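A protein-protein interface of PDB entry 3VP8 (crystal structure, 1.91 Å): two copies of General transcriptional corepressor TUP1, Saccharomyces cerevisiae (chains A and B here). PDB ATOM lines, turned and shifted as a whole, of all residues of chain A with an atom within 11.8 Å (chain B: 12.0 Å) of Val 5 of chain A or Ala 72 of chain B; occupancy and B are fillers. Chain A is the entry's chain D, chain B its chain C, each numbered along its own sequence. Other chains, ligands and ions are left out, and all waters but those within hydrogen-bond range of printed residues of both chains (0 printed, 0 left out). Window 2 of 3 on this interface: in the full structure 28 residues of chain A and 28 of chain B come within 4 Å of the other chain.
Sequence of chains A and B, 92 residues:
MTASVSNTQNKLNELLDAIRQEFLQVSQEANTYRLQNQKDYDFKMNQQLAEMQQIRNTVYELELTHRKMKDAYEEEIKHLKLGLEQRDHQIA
The side-chain amide nitrogen (NE2) of Gln 9 of chain A sits at hydrogen-bond distance from the side-chain amide oxygen (OD1) of Asn 13 of chain A, 3.1 Å away.
Among the printed residues, merely in contact across the chains: Val 5 of chain A with Met 69 of chain B (3.5 Å), Val 5 of chain A with Ala 72 of chain B (3.8 Å), Val 5 of chain A with Tyr 73 of chain B (3.98 Å), Thr 8 of chain A with Thr 65 of chain B (3.8 Å), Thr 8 of chain A with Met 69 of chain B (3.2 Å), Gln 9 of chain A with Met 69 of chain B (3.5 Å), Lys 11 of chain A with Thr 65 of chain B (3.9 Å), Leu 12 of chain A with Leu 62 of chain B (3.99 Å), Leu 12 of chain A with Thr 65 of chain B (3.2 Å), Leu 12 of chain A with His 66 of chain B (3.4 Å), Leu 12 of chain A with Met 69 of chain B (3.9 Å), Leu 15 of chain A with Leu 62 of chain B (3.5 Å) and Leu 15 of chain A with Thr 65 of chain B (3.5 Å).
No residue of chain B comes within 4 Å of Thr 2 of chain A.
No residue of chain B comes within 4 Å of Ala 3 of chain A.
Of chain B, only Met 69 (3.5 Å), Ala 72 (3.8 Å) and Tyr 73 (3.98 Å) come within 4 Å of Val 5 of chain A.
No residue of chain B comes within 4 Å of Asn 7 of chain A.
Thr 8 of chain A touches two residues of chain B.
Printed residues of chain B within 4 Å of Lys 11 of chain A: Thr 65.
Of the printed residues of chain A, Leu 62 of chain B touches Leu 12 (3.99 Å) and Leu 15 (3.5 Å).
No residue of chain A comes within 4 Å of Asp 71 of chain B.
Of chain A, only Val 5 (3.8 Å) comes within 4 Å of Ala 72 of chain B.
Of chain A, only Val 5 comes within 4 Å of Tyr 73 of chain B.
Glu 74 of chain B touches none of the printed residues of chain A.
The nearest residue of chain A that does not touch Ala 72 of chain B is Ser 4 of chain A (4.7 Å).
Of the 19 printed residues of chain B, 6 touch a printed residue of chain A.
Printed residues of chain B that touch a printed residue of chain A: Leu 62, Thr 65, His 66, Met 69, Ala 72 and Tyr 73.
Printed residues of chain A that touch a printed residue of chain B: Val 5, Thr 8, Gln 9, Lys 11, Leu 12 and Leu 15.
Hydrophobic or aromatic side chains of chain A within 4 Å of the printed part of chain B: Val 5, Leu 12 and Leu 15.
Along chain A the printed residues that touch a printed residue of chain B span positions 5 to 15.
No position is printed for both chains.
Of the 13 pairs that touch across the chains among the printed residues, none has its exchanged pair printed and touching as well.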
ATOM      1  N   THR A   2      29.869  -3.501  24.668  1.00  0.00           N
ATOM      2  CA  THR A   2      29.311  -4.848  24.763  1.00  0.00           C
ATOM      3  C   THR A   2      29.884  -5.763  23.681  1.00  0.00           C
ATOM      4  O   THR A   2      30.380  -5.293  22.661  1.00  0.00           O
ATOM      5  CB  THR A   2      27.773  -4.832  24.638  1.00  0.00           C
ATOM      6  OG1 THR A   2      27.262  -6.169  24.710  1.00  0.00           O
ATOM      7  CG2 THR A   2      27.357  -4.212  23.315  1.00  0.00           C
ATOM      8  N   ALA A   3      29.825  -7.069  23.916  1.00  0.00           N
ATOM      9  CA  ALA A   3      30.240  -8.050  22.917  1.00  0.00           C
ATOM     10  C   ALA A   3      29.082  -8.321  21.960  1.00  0.00           C
ATOM     11  O   ALA A   3      29.282  -8.683  20.793  1.00  0.00           O
ATOM     12  CB  ALA A   3      30.687  -9.339  23.596  1.00  0.00           C
ATOM     13  N   SER A   4      27.867  -8.132  22.467  1.00  0.00           N
ATOM     14  CA  SER A   4      26.652  -8.469  21.730  1.00  0.00           C
ATOM     15  C   SER A   4      26.411  -7.573  20.514  1.00  0.00           C
ATOM     16  O   SER A   4      26.046  -8.062  19.446  1.00  0.00           O
ATOM     17  CB  SER A   4      25.442  -8.427  22.664  1.00  0.00           C
ATOM     18  OG  SER A   4      24.378  -7.689  22.090  1.00  0.00           O
ATOM     19  N   VAL A   5      26.592  -6.265  20.681  1.00  0.00           N
ATOM     20  CA  VAL A   5      26.409  -5.326  19.577  1.00  0.00           C
ATOM     21  C   VAL A   5      27.295  -5.708  18.396  1.00  0.00           C
ATOM     22  O   VAL A   5      26.927  -5.490  17.242  1.00  0.00           O
ATOM     23  CB  VAL A   5      26.659  -3.857  20.009  1.00  0.00           C
ATOM     24  CG1 VAL A   5      27.058  -3.004  18.822  1.00  0.00           C
ATOM     25  CG2 VAL A   5      25.418  -3.285  20.682  1.00  0.00           C
ATOM     26  N   SER A   6      28.447  -6.302  18.691  1.00  0.00           N
ATOM     27  CA  SER A   6      29.356  -6.787  17.658  1.00  0.00           C
ATOM     28  C   SER A   6      28.714  -7.925  16.872  1.00  0.00           C
ATOM     29  O   SER A   6      28.908  -8.050  15.665  1.00  0.00           O
ATOM     30  CB  SER A   6      30.673  -7.263  18.284  1.00  0.00           C
ATOM     31  OG  SER A   6      31.362  -6.184  18.886  1.00  0.00           O
ATOM     32  N   ASN A   7      27.947  -8.755  17.570  1.00  0.00           N
ATOM     33  CA  ASN A   7      27.347  -9.927  16.953  1.00  0.00           C
ATOM     34  C   ASN A   7      26.071  -9.617  16.195  1.00  0.00           C
ATOM     35  O   ASN A   7      25.749 -10.302  15.220  1.00  0.00           O
ATOM     36  CB  ASN A   7      27.109 -11.031  17.986  1.00  0.00           C
ATOM     37  CG  ASN A   7      28.401 -11.690  18.437  1.00  0.00           C
ATOM     38  OD1 ASN A   7      29.425 -11.612  17.755  1.00  0.00           O
ATOM     39  ND2 ASN A   7      28.357 -12.350  19.590  1.00  0.00           N
ATOM     40  N   THR A   8      25.335  -8.599  16.633  1.00  0.00           N
ATOM     41  CA  THR A   8      24.162  -8.201  15.867  1.00  0.00           C
ATOM     42  C   THR A   8      24.630  -7.448  14.631  1.00  0.00           C
ATOM     43  O   THR A   8      24.078  -7.627  13.553  1.00  0.00           O
ATOM     44  CB  THR A   8      23.149  -7.379  16.679  1.00  0.00           C
ATOM     45  OG1 THR A   8      23.499  -5.994  16.623  1.00  0.00           O
ATOM     46  CG2 THR A   8      23.122  -7.857  18.116  1.00  0.00           C
ATOM     47  N   GLN A   9      25.661  -6.621  14.779  1.00  0.00           N
ATOM     48  CA  GLN A   9      26.278  -6.009  13.607  1.00  0.00           C
ATOM     49  C   GLN A   9      26.814  -7.091  12.661  1.00  0.00           C
ATOM     50  O   GLN A   9      26.978  -6.853  11.455  1.00  0.00           O
ATOM     51  CB  GLN A   9      27.398  -5.055  14.002  1.00  0.00           C
ATOM     52  CG  GLN A   9      27.972  -4.260  12.826  1.00  0.00           C
ATOM     53  CD  GLN A   9      26.935  -3.387  12.144  1.00  0.00           C
ATOM     54  OE1 GLN A   9      26.288  -2.551  12.787  1.00  0.00           O
ATOM     55  NE2 GLN A   9      26.762  -3.581  10.836  1.00  0.00           N
ATOM     56  N   ASN A  10      27.085  -8.272  13.218  1.00  0.00           N
ATOM     57  CA  ASN A  10      27.556  -9.419  12.446  1.00  0.00           C
ATOM     58  C   ASN A  10      26.452  -9.990  11.600  1.00  0.00           C
ATOM     59  O   ASN A  10      26.577 -10.096  10.378  1.00  0.00           O
ATOM     60  CB  ASN A  10      28.070 -10.525  13.369  1.00  0.00           C
ATOM     61  CG  ASN A  10      29.528 -10.359  13.722  1.00  0.00           C
ATOM     62  OD1 ASN A  10      30.259  -9.604  13.071  1.00  0.00           O
ATOM     63  ND2 ASN A  10      29.969 -11.078  14.754  1.00  0.00           N
ATOM     64  N   LYS A  11      25.384 -10.402  12.271  1.00  0.00           N
ATOM     65  CA  LYS A  11      24.221 -10.901  11.579  1.00  0.00           C
ATOM     66  C   LYS A  11      23.833  -9.887  10.508  1.00  0.00           C
ATOM     67  O   LYS A  11      23.606 -10.257   9.363  1.00  0.00           O
ATOM     68  CB  LYS A  11      23.070 -11.156  12.553  1.00  0.00           C
ATOM     69  CG  LYS A  11      22.229 -12.358  12.146  1.00  0.00           C
ATOM     70  CD  LYS A  11      21.220 -12.765  13.209  1.00  0.00           C
ATOM     71  CE  LYS A  11      20.438 -13.997  12.747  1.00  0.00           C
ATOM     72  NZ  LYS A  11      19.111 -14.112  13.424  1.00  0.00           N
ATOM     73  N   LEU A  12      23.804  -8.607  10.870  1.00  0.00           N
ATOM     74  CA  LEU A  12      23.432  -7.562   9.920  1.00  0.00           C
ATOM     75  C   LEU A  12      24.256  -7.628   8.644  1.00  0.00           C
ATOM     76  O   LEU A  12      23.711  -7.660   7.542  1.00  0.00           O
ATOM     77  CB  LEU A  12      23.578  -6.175  10.540  1.00  0.00           C
ATOM     78  CG  LEU A  12      22.446  -5.708  11.451  1.00  0.00           C
ATOM     79  CD1 LEU A  12      22.818  -4.363  12.090  1.00  0.00           C
ATOM     80  CD2 LEU A  12      21.137  -5.613  10.662  1.00  0.00           C
ATOM     81  N   ASN A  13      25.573  -7.633   8.790  1.00  0.00           N
ATOM     82  CA  ASN A  13      26.434  -7.615   7.622  1.00  0.00           C
ATOM     83  C   ASN A  13      26.230  -8.865   6.779  1.00  0.00           C
ATOM     84  O   ASN A  13      26.317  -8.817   5.553  1.00  0.00           O
ATOM     85  CB  ASN A  13      27.901  -7.439   8.024  1.00  0.00           C
ATOM     86  CG  ASN A  13      28.194  -6.048   8.549  1.00  0.00           C
ATOM     87  OD1 ASN A  13      27.462  -5.097   8.260  1.00  0.00           O
ATOM     88  ND2 ASN A  13      29.272  -5.917   9.321  1.00  0.00           N
ATOM     89  N   GLU A  14      25.924  -9.971   7.450  1.00  0.00           N
ATOM     90  CA  GLU A  14      25.718 -11.261   6.801  1.00  0.00           C
ATOM     91  C   GLU A  14      24.350 -11.348   6.109  1.00  0.00           C
ATOM     92  O   GLU A  14      24.237 -11.860   4.990  1.00  0.00           O
ATOM     93  CB  GLU A  14      25.837 -12.385   7.825  1.00  0.00           C
ATOM     94  CG  GLU A  14      24.846 -13.522   7.608  1.00  0.00           C
ATOM     95  CD  GLU A  14      24.687 -14.392   8.837  1.00  0.00           C
ATOM     96  OE1 GLU A  14      23.714 -15.181   8.894  1.00  0.00           O
ATOM     97  OE2 GLU A  14      25.538 -14.286   9.752  1.00  0.00           O
ATOM     98  N   LEU A  15      23.316 -10.872   6.794  1.00  0.00           N
ATOM     99  CA  LEU A  15      21.995 -10.775   6.203  1.00  0.00           C
ATOM    100  C   LEU A  15      22.042  -9.905   4.948  1.00  0.00           C
ATOM    101  O   LEU A  15      21.422 -10.232   3.934  1.00  0.00           O
ATOM    102  CB  LEU A  15      21.014 -10.193   7.220  1.00  0.00           C
ATOM    103  CG  LEU A  15      20.744 -11.115   8.409  1.00  0.00           C
ATOM    104  CD1 LEU A  15      19.896 -10.430   9.489  1.00  0.00           C
ATOM    105  CD2 LEU A  15      20.078 -12.403   7.930  1.00  0.00           C
ATOM    106  N   LEU B  62      16.381  -8.904   8.894  1.00  0.00           N
ATOM    107  CA  LEU B  62      17.136  -7.658   9.006  1.00  0.00           C
ATOM    108  C   LEU B  62      16.463  -6.783  10.049  1.00  0.00           C
ATOM    109  O   LEU B  62      17.108  -6.310  10.979  1.00  0.00           O
ATOM    110  CB  LEU B  62      17.209  -6.911   7.676  1.00  0.00           C
ATOM    111  CG  LEU B  62      18.291  -7.385   6.703  1.00  0.00           C
ATOM    112  CD1 LEU B  62      18.051  -6.838   5.287  1.00  0.00           C
ATOM    113  CD2 LEU B  62      19.678  -6.988   7.207  1.00  0.00           C
ATOM    114  N   GLU B  63      15.154  -6.602   9.895  1.00  0.00           N
ATOM    115  CA  GLU B  63      14.356  -5.790  10.813  1.00  0.00           C
ATOM    116  C   GLU B  63      14.465  -6.252  12.256  1.00  0.00           C
ATOM    117  O   GLU B  63      14.540  -5.429  13.173  1.00  0.00           O
ATOM    118  CB  GLU B  63      12.891  -5.784  10.372  1.00  0.00           C
ATOM    119  CG  GLU B  63      12.634  -4.794   9.254  1.00  0.00           C
ATOM    120  CD  GLU B  63      13.060  -3.390   9.648  1.00  0.00           C
ATOM    121  OE1 GLU B  63      13.760  -2.711   8.865  1.00  0.00           O
ATOM    122  OE2 GLU B  63      12.691  -2.968  10.758  1.00  0.00           O
ATOM    123  N   LEU B  64      14.469  -7.566  12.453  1.00  0.00           N
ATOM    124  CA  LEU B  64      14.595  -8.143  13.785  1.00  0.00           C
ATOM    125  C   LEU B  64      15.923  -7.778  14.427  1.00  0.00           C
ATOM    126  O   LEU B  64      15.959  -7.269  15.557  1.00  0.00           O
ATOM    127  CB  LEU B  64      14.473  -9.662  13.717  1.00  0.00           C
ATOM    128  CG  LEU B  64      13.303 -10.328  14.435  1.00  0.00           C
ATOM    129  CD1 LEU B  64      11.996 -10.079  13.691  1.00  0.00           C
ATOM    130  CD2 LEU B  64      13.570 -11.822  14.580  1.00  0.00           C
ATOM    131  N   THR B  65      17.026  -8.034  13.726  1.00  0.00           N
ATOM    132  CA  THR B  65      18.322  -7.773  14.349  1.00  0.00           C
ATOM    133  C   THR B  65      18.631  -6.277  14.471  1.00  0.00           C
ATOM    134  O   THR B  65      19.386  -5.870  15.356  1.00  0.00           O
ATOM    135  CB  THR B  65      19.484  -8.567  13.706  1.00  0.00           C
ATOM    136  OG1 THR B  65      20.355  -7.678  13.005  1.00  0.00           O
ATOM    137  CG2 THR B  65      18.944  -9.652  12.768  1.00  0.00           C
ATOM    138  N   HIS B  66      18.050  -5.464  13.593  1.00  0.00           N
ATOM    139  CA  HIS B  66      18.096  -4.014  13.781  1.00  0.00           C
ATOM    140  C   HIS B  66      17.416  -3.615  15.097  1.00  0.00           C
ATOM    141  O   HIS B  66      17.946  -2.795  15.844  1.00  0.00           O
ATOM    142  CB  HIS B  66      17.476  -3.272  12.597  1.00  0.00           C
ATOM    143  CG  HIS B  66      18.439  -3.000  11.492  1.00  0.00           C
ATOM    144  ND1 HIS B  66      19.648  -2.359  11.695  1.00  0.00           N
ATOM    145  CD2 HIS B  66      18.386  -3.276  10.166  1.00  0.00           C
ATOM    146  CE1 HIS B  66      20.289  -2.258  10.548  1.00  0.00           C
ATOM    147  NE2 HIS B  66      19.547  -2.802   9.604  1.00  0.00           N
ATOM    148  N   ARG B  67      16.259  -4.209  15.378  1.00  0.00           N
ATOM    149  CA  ARG B  67      15.566  -4.023  16.657  1.00  0.00           C
ATOM    150  C   ARG B  67      16.358  -4.550  17.856  1.00  0.00           C
ATOM    151  O   ARG B  67      16.240  -4.027  18.974  1.00  0.00           O
ATOM    152  CB  ARG B  67      14.180  -4.676  16.616  1.00  0.00           C
ATOM    153  CG  ARG B  67      13.058  -3.728  16.219  1.00  0.00           C
ATOM    154  CD  ARG B  67      11.837  -4.473  15.685  1.00  0.00           C
ATOM    155  NE  ARG B  67      11.493  -4.035  14.331  1.00  0.00           N
ATOM    156  CZ  ARG B  67      10.661  -4.677  13.514  1.00  0.00           C
ATOM    157  NH1 ARG B  67      10.068  -5.800  13.904  1.00  0.00           N
ATOM    158  NH2 ARG B  67      10.423  -4.195  12.298  1.00  0.00           N
ATOM    159  N   LYS B  68      17.152  -5.588  17.631  1.00  0.00           N
ATOM    160  CA  LYS B  68      18.040  -6.097  18.670  1.00  0.00           C
ATOM    161  C   LYS B  68      19.188  -5.128  18.925  1.00  0.00           C
ATOM    162  O   LYS B  68      19.634  -4.959  20.064  1.00  0.00           O
ATOM    163  CB  LYS B  68      18.583  -7.475  18.287  1.00  0.00           C
ATOM    164  CG  LYS B  68      17.920  -8.623  19.025  1.00  0.00           C
ATOM    165  CD  LYS B  68      16.402  -8.463  19.075  1.00  0.00           C
ATOM    166  CE  LYS B  68      15.748  -9.586  19.885  1.00  0.00           C
ATOM    167  NZ  LYS B  68      15.300  -9.162  21.250  1.00  0.00           N
ATOM    168  N   MET B  69      19.665  -4.490  17.859  1.00  0.00           N
ATOM    169  CA  MET B  69      20.722  -3.495  17.982  1.00  0.00           C
ATOM    170  C   MET B  69      20.205  -2.257  18.702  1.00  0.00           C
ATOM    171  O   MET B  69      20.830  -1.777  19.646  1.00  0.00           O
ATOM    172  CB  MET B  69      21.289  -3.125  16.615  1.00  0.00           C
ATOM    173  CG  MET B  69      22.327  -2.043  16.677  1.00  0.00           C
ATOM    174  SD  MET B  69      23.414  -2.106  15.250  1.00  0.00           S
ATOM    175  CE  MET B  69      24.743  -3.129  15.901  1.00  0.00           C
ATOM    176  N   LYS B  70      19.057  -1.756  18.255  1.00  0.00           N
ATOM    177  CA  LYS B  70      18.384  -0.649  18.915  1.00  0.00           C
ATOM    178  C   LYS B  70      18.164  -0.946  20.398  1.00  0.00           C
ATOM    179  O   LYS B  70      18.607  -0.182  21.265  1.00  0.00           O
ATOM    180  CB  LYS B  70      17.057  -0.353  18.215  1.00  0.00           C
ATOM    181  CG  LYS B  70      16.150   0.602  18.967  1.00  0.00           C
ATOM    182  CD  LYS B  70      15.320   1.444  18.010  1.00  0.00           C
ATOM    183  CE  LYS B  70      14.147   2.098  18.737  1.00  0.00           C
ATOM    184  NZ  LYS B  70      13.724   3.355  18.054  1.00  0.00           N
ATOM    185  N   ASP B  71      17.500  -2.063  20.690  1.00  0.00           N
ATOM    186  CA  ASP B  71      17.261  -2.475  22.078  1.00  0.00           C
ATOM    187  C   ASP B  71      18.522  -2.431  22.951  1.00  0.00           C
ATOM    188  O   ASP B  71      18.465  -2.018  24.119  1.00  0.00           O
ATOM    189  CB  ASP B  71      16.636  -3.872  22.126  1.00  0.00           C
ATOM    190  CG  ASP B  71      15.148  -3.858  21.830  1.00  0.00           C
ATOM    191  OD1 ASP B  71      14.605  -2.774  21.513  1.00  0.00           O
ATOM    192  OD2 ASP B  71      14.520  -4.938  21.907  1.00  0.00           O
ATOM    193  N   ALA B  72      19.652  -2.850  22.383  1.00  0.00           N
ATOM    194  CA  ALA B  72      20.925  -2.853  23.095  1.00  0.00           C
ATOM    195  C   ALA B  72      21.414  -1.427  23.376  1.00  0.00           C
ATOM    196  O   ALA B  72      21.803  -1.102  24.498  1.00  0.00           O
ATOM    197  CB  ALA B  72      21.966  -3.629  22.310  1.00  0.00           C
ATOM    198  N   TYR B  73      21.395  -0.582  22.351  1.00  0.00           N
ATOM    199  CA  TYR B  73      21.743   0.825  22.509  1.00  0.00           C
ATOM    200  C   TYR B  73      20.840   1.483  23.538  1.00  0.00           C
ATOM    201  O   TYR B  73      21.240   2.438  24.214  1.00  0.00           O
ATOM    202  CB  TYR B  73      21.635   1.553  21.166  1.00  0.00           C
ATOM    203  CG  TYR B  73      22.856   1.402  20.282  1.00  0.00           C
ATOM    204  CD1 TYR B  73      23.149   0.195  19.664  1.00  0.00           C
ATOM    205  CD2 TYR B  73      23.709   2.469  20.064  1.00  0.00           C
ATOM    206  CE1 TYR B  73      24.266   0.059  18.862  1.00  0.00           C
ATOM    207  CE2 TYR B  73      24.827   2.344  19.268  1.00  0.00           C
ATOM    208  CZ  TYR B  73      25.104   1.137  18.667  1.00  0.00           C
ATOM    209  OH  TYR B  73      26.219   1.011  17.861  1.00  0.00           O
ATOM    210  N   GLU B  74      19.617   0.973  23.651  1.00  0.00           N
ATOM    211  CA  GLU B  74      18.659   1.507  24.614  1.00  0.00           C
ATOM    212  C   GLU B  74      19.016   1.110  26.049  1.00  0.00           C
ATOM    213  O   GLU B  74      18.673   1.822  26.997  1.00  0.00           O
ATOM    214  CB  GLU B  74      17.218   1.106  24.261  1.00  0.00           C
ATOM    215  CG  GLU B  74      16.613   1.922  23.110  1.00  0.00           C
ATOM    216  CD  GLU B  74      15.161   1.562  22.803  1.00  0.00           C
ATOM    217  OE1 GLU B  74      14.774   0.384  22.966  1.00  0.00           O
ATOM    218  OE2 GLU B  74      14.400   2.464  22.386  1.00  0.00           O
ATOM    219  N   GLU B  75      19.704  -0.016  26.210  1.00  0.00           N
ATOM    220  CA  GLU B  75      20.137  -0.449  27.535  1.00  0.00           C
ATOM    221  C   GLU B  75      21.317   0.385  28.032  1.00  0.00           C
ATOM    222  O   GLU B  75      21.414   0.674  29.222  1.00  0.00           O
ATOM    223  CB  GLU B  75      20.488  -1.937  27.549  1.00  0.00           C
ATOM    224  CG  GLU B  75      19.291  -2.873  27.689  1.00  0.00           C
ATOM    225  CD  GLU B  75      18.485  -2.627  28.963  1.00  0.00           C
ATOM    226  OE1 GLU B  75      17.500  -1.856  28.911  1.00  0.00           O
ATOM    227  OE2 GLU B  75      18.828  -3.208  30.016  1.00  0.00           O
ATOM    228  N   GLU B  76      22.210   0.768  27.123  1.00  0.00           N
ATOM    229  CA  GLU B  76      23.334   1.632  27.475  1.00  0.00           C
ATOM    230  C   GLU B  76      22.842   3.030  27.838  1.00  0.00           C
ATOM    231  O   GLU B  76      23.126   3.535  28.921  1.00  0.00           O
ATOM    232  CB  GLU B  76      24.331   1.708  26.324  1.00  0.00           C
ATOM    233  CG  GLU B  76      24.928   0.373  25.953  1.00  0.00           C
ATOM    234  CD  GLU B  76      26.431   0.356  26.120  1.00  0.00           C
ATOM    235  OE1 GLU B  76      27.139   0.528  25.105  1.00  0.00           O
ATOM    236  OE2 GLU B  76      26.906   0.178  27.266  1.00  0.00           O
ATOM    237  N   ILE B  77      22.107   3.654  26.923  1.00  0.00           N
ATOM    238  CA  ILE B  77      21.473   4.937  27.206  1.00  0.00           C
ATOM    239  C   ILE B  77      20.768   4.908  28.567  1.00  0.00           C
ATOM    240  O   ILE B  77      20.660   5.937  29.238  1.00  0.00           O
ATOM    241  CB  ILE B  77      20.471   5.328  26.098  1.00  0.00           C
ATOM    242  CG1 ILE B  77      21.210   5.781  24.836  1.00  0.00           C
ATOM    243  CG2 ILE B  77      19.532   6.432  26.567  1.00  0.00           C
ATOM    244  CD1 ILE B  77      20.351   6.603  23.898  1.00  0.00           C
ATOM    245  N   LYS B  78      20.298   3.725  28.966  1.00  0.00           N
ATOM    246  CA  LYS B  78      19.651   3.520  30.262  1.00  0.00           C
ATOM    247  C   LYS B  78      20.682   3.400  31.377  1.00  0.00           C
ATOM    248  O   LYS B  78      20.681   4.192  32.318  1.00  0.00           O
ATOM    249  CB  LYS B  78      18.782   2.257  30.234  1.00  0.00           C
ATOM    250  CG  LYS B  78      17.284   2.507  30.333  1.00  0.00           C
ATOM    251  CD  LYS B  78      16.637   1.407  31.169  1.00  0.00           C
ATOM    252  CE  LYS B  78      15.291   0.991  30.597  1.00  0.00           C
ATOM    253  NZ  LYS B  78      15.001  -0.443  30.890  1.00  0.00           N
ATOM    254  N   HIS B  79      21.532   2.380  31.276  1.00  0.00           N
ATOM    255  CA  HIS B  79      22.680   2.196  32.161  1.00  0.00           C
ATOM    256  C   HIS B  79      23.267   3.531  32.589  1.00  0.00           C
ATOM    257  O   HIS B  79      23.330   3.859  33.778  1.00  0.00           O
ATOM    258  CB  HIS B  79      23.800   1.444  31.425  1.00  0.00           C
ATOM    259  CG  HIS B  79      23.715  -0.048  31.513  1.00  0.00           C
ATOM    260  ND1 HIS B  79      24.798  -0.869  31.264  1.00  0.00           N
ATOM    261  CD2 HIS B  79      22.683  -0.872  31.820  1.00  0.00           C
ATOM    262  CE1 HIS B  79      24.437  -2.126  31.419  1.00  0.00           C
ATOM    263  NE2 HIS B  79      23.161  -2.160  31.754  1.00  0.00           N
ATOM    264  N   LEU B  80      23.693   4.298  31.590  1.00  0.00           N
ATOM    265  CA  LEU B  80      24.595   5.426  31.796  1.00  0.00           C
ATOM    266  C   LEU B  80      24.059   6.486  32.752  1.00  0.00           C
ATOM    267  O   LEU B  80      24.793   7.391  33.151  1.00  0.00           O
ATOM    268  CB  LEU B  80      25.013   6.034  30.447  1.00  0.00           C
ATOM    269  CG  LEU B  80      25.709   5.043  29.506  1.00  0.00           C
ATOM    270  CD1 LEU B  80      26.139   5.696  28.194  1.00  0.00           C
ATOM    271  CD2 LEU B  80      26.899   4.402  30.208  1.00  0.00           C
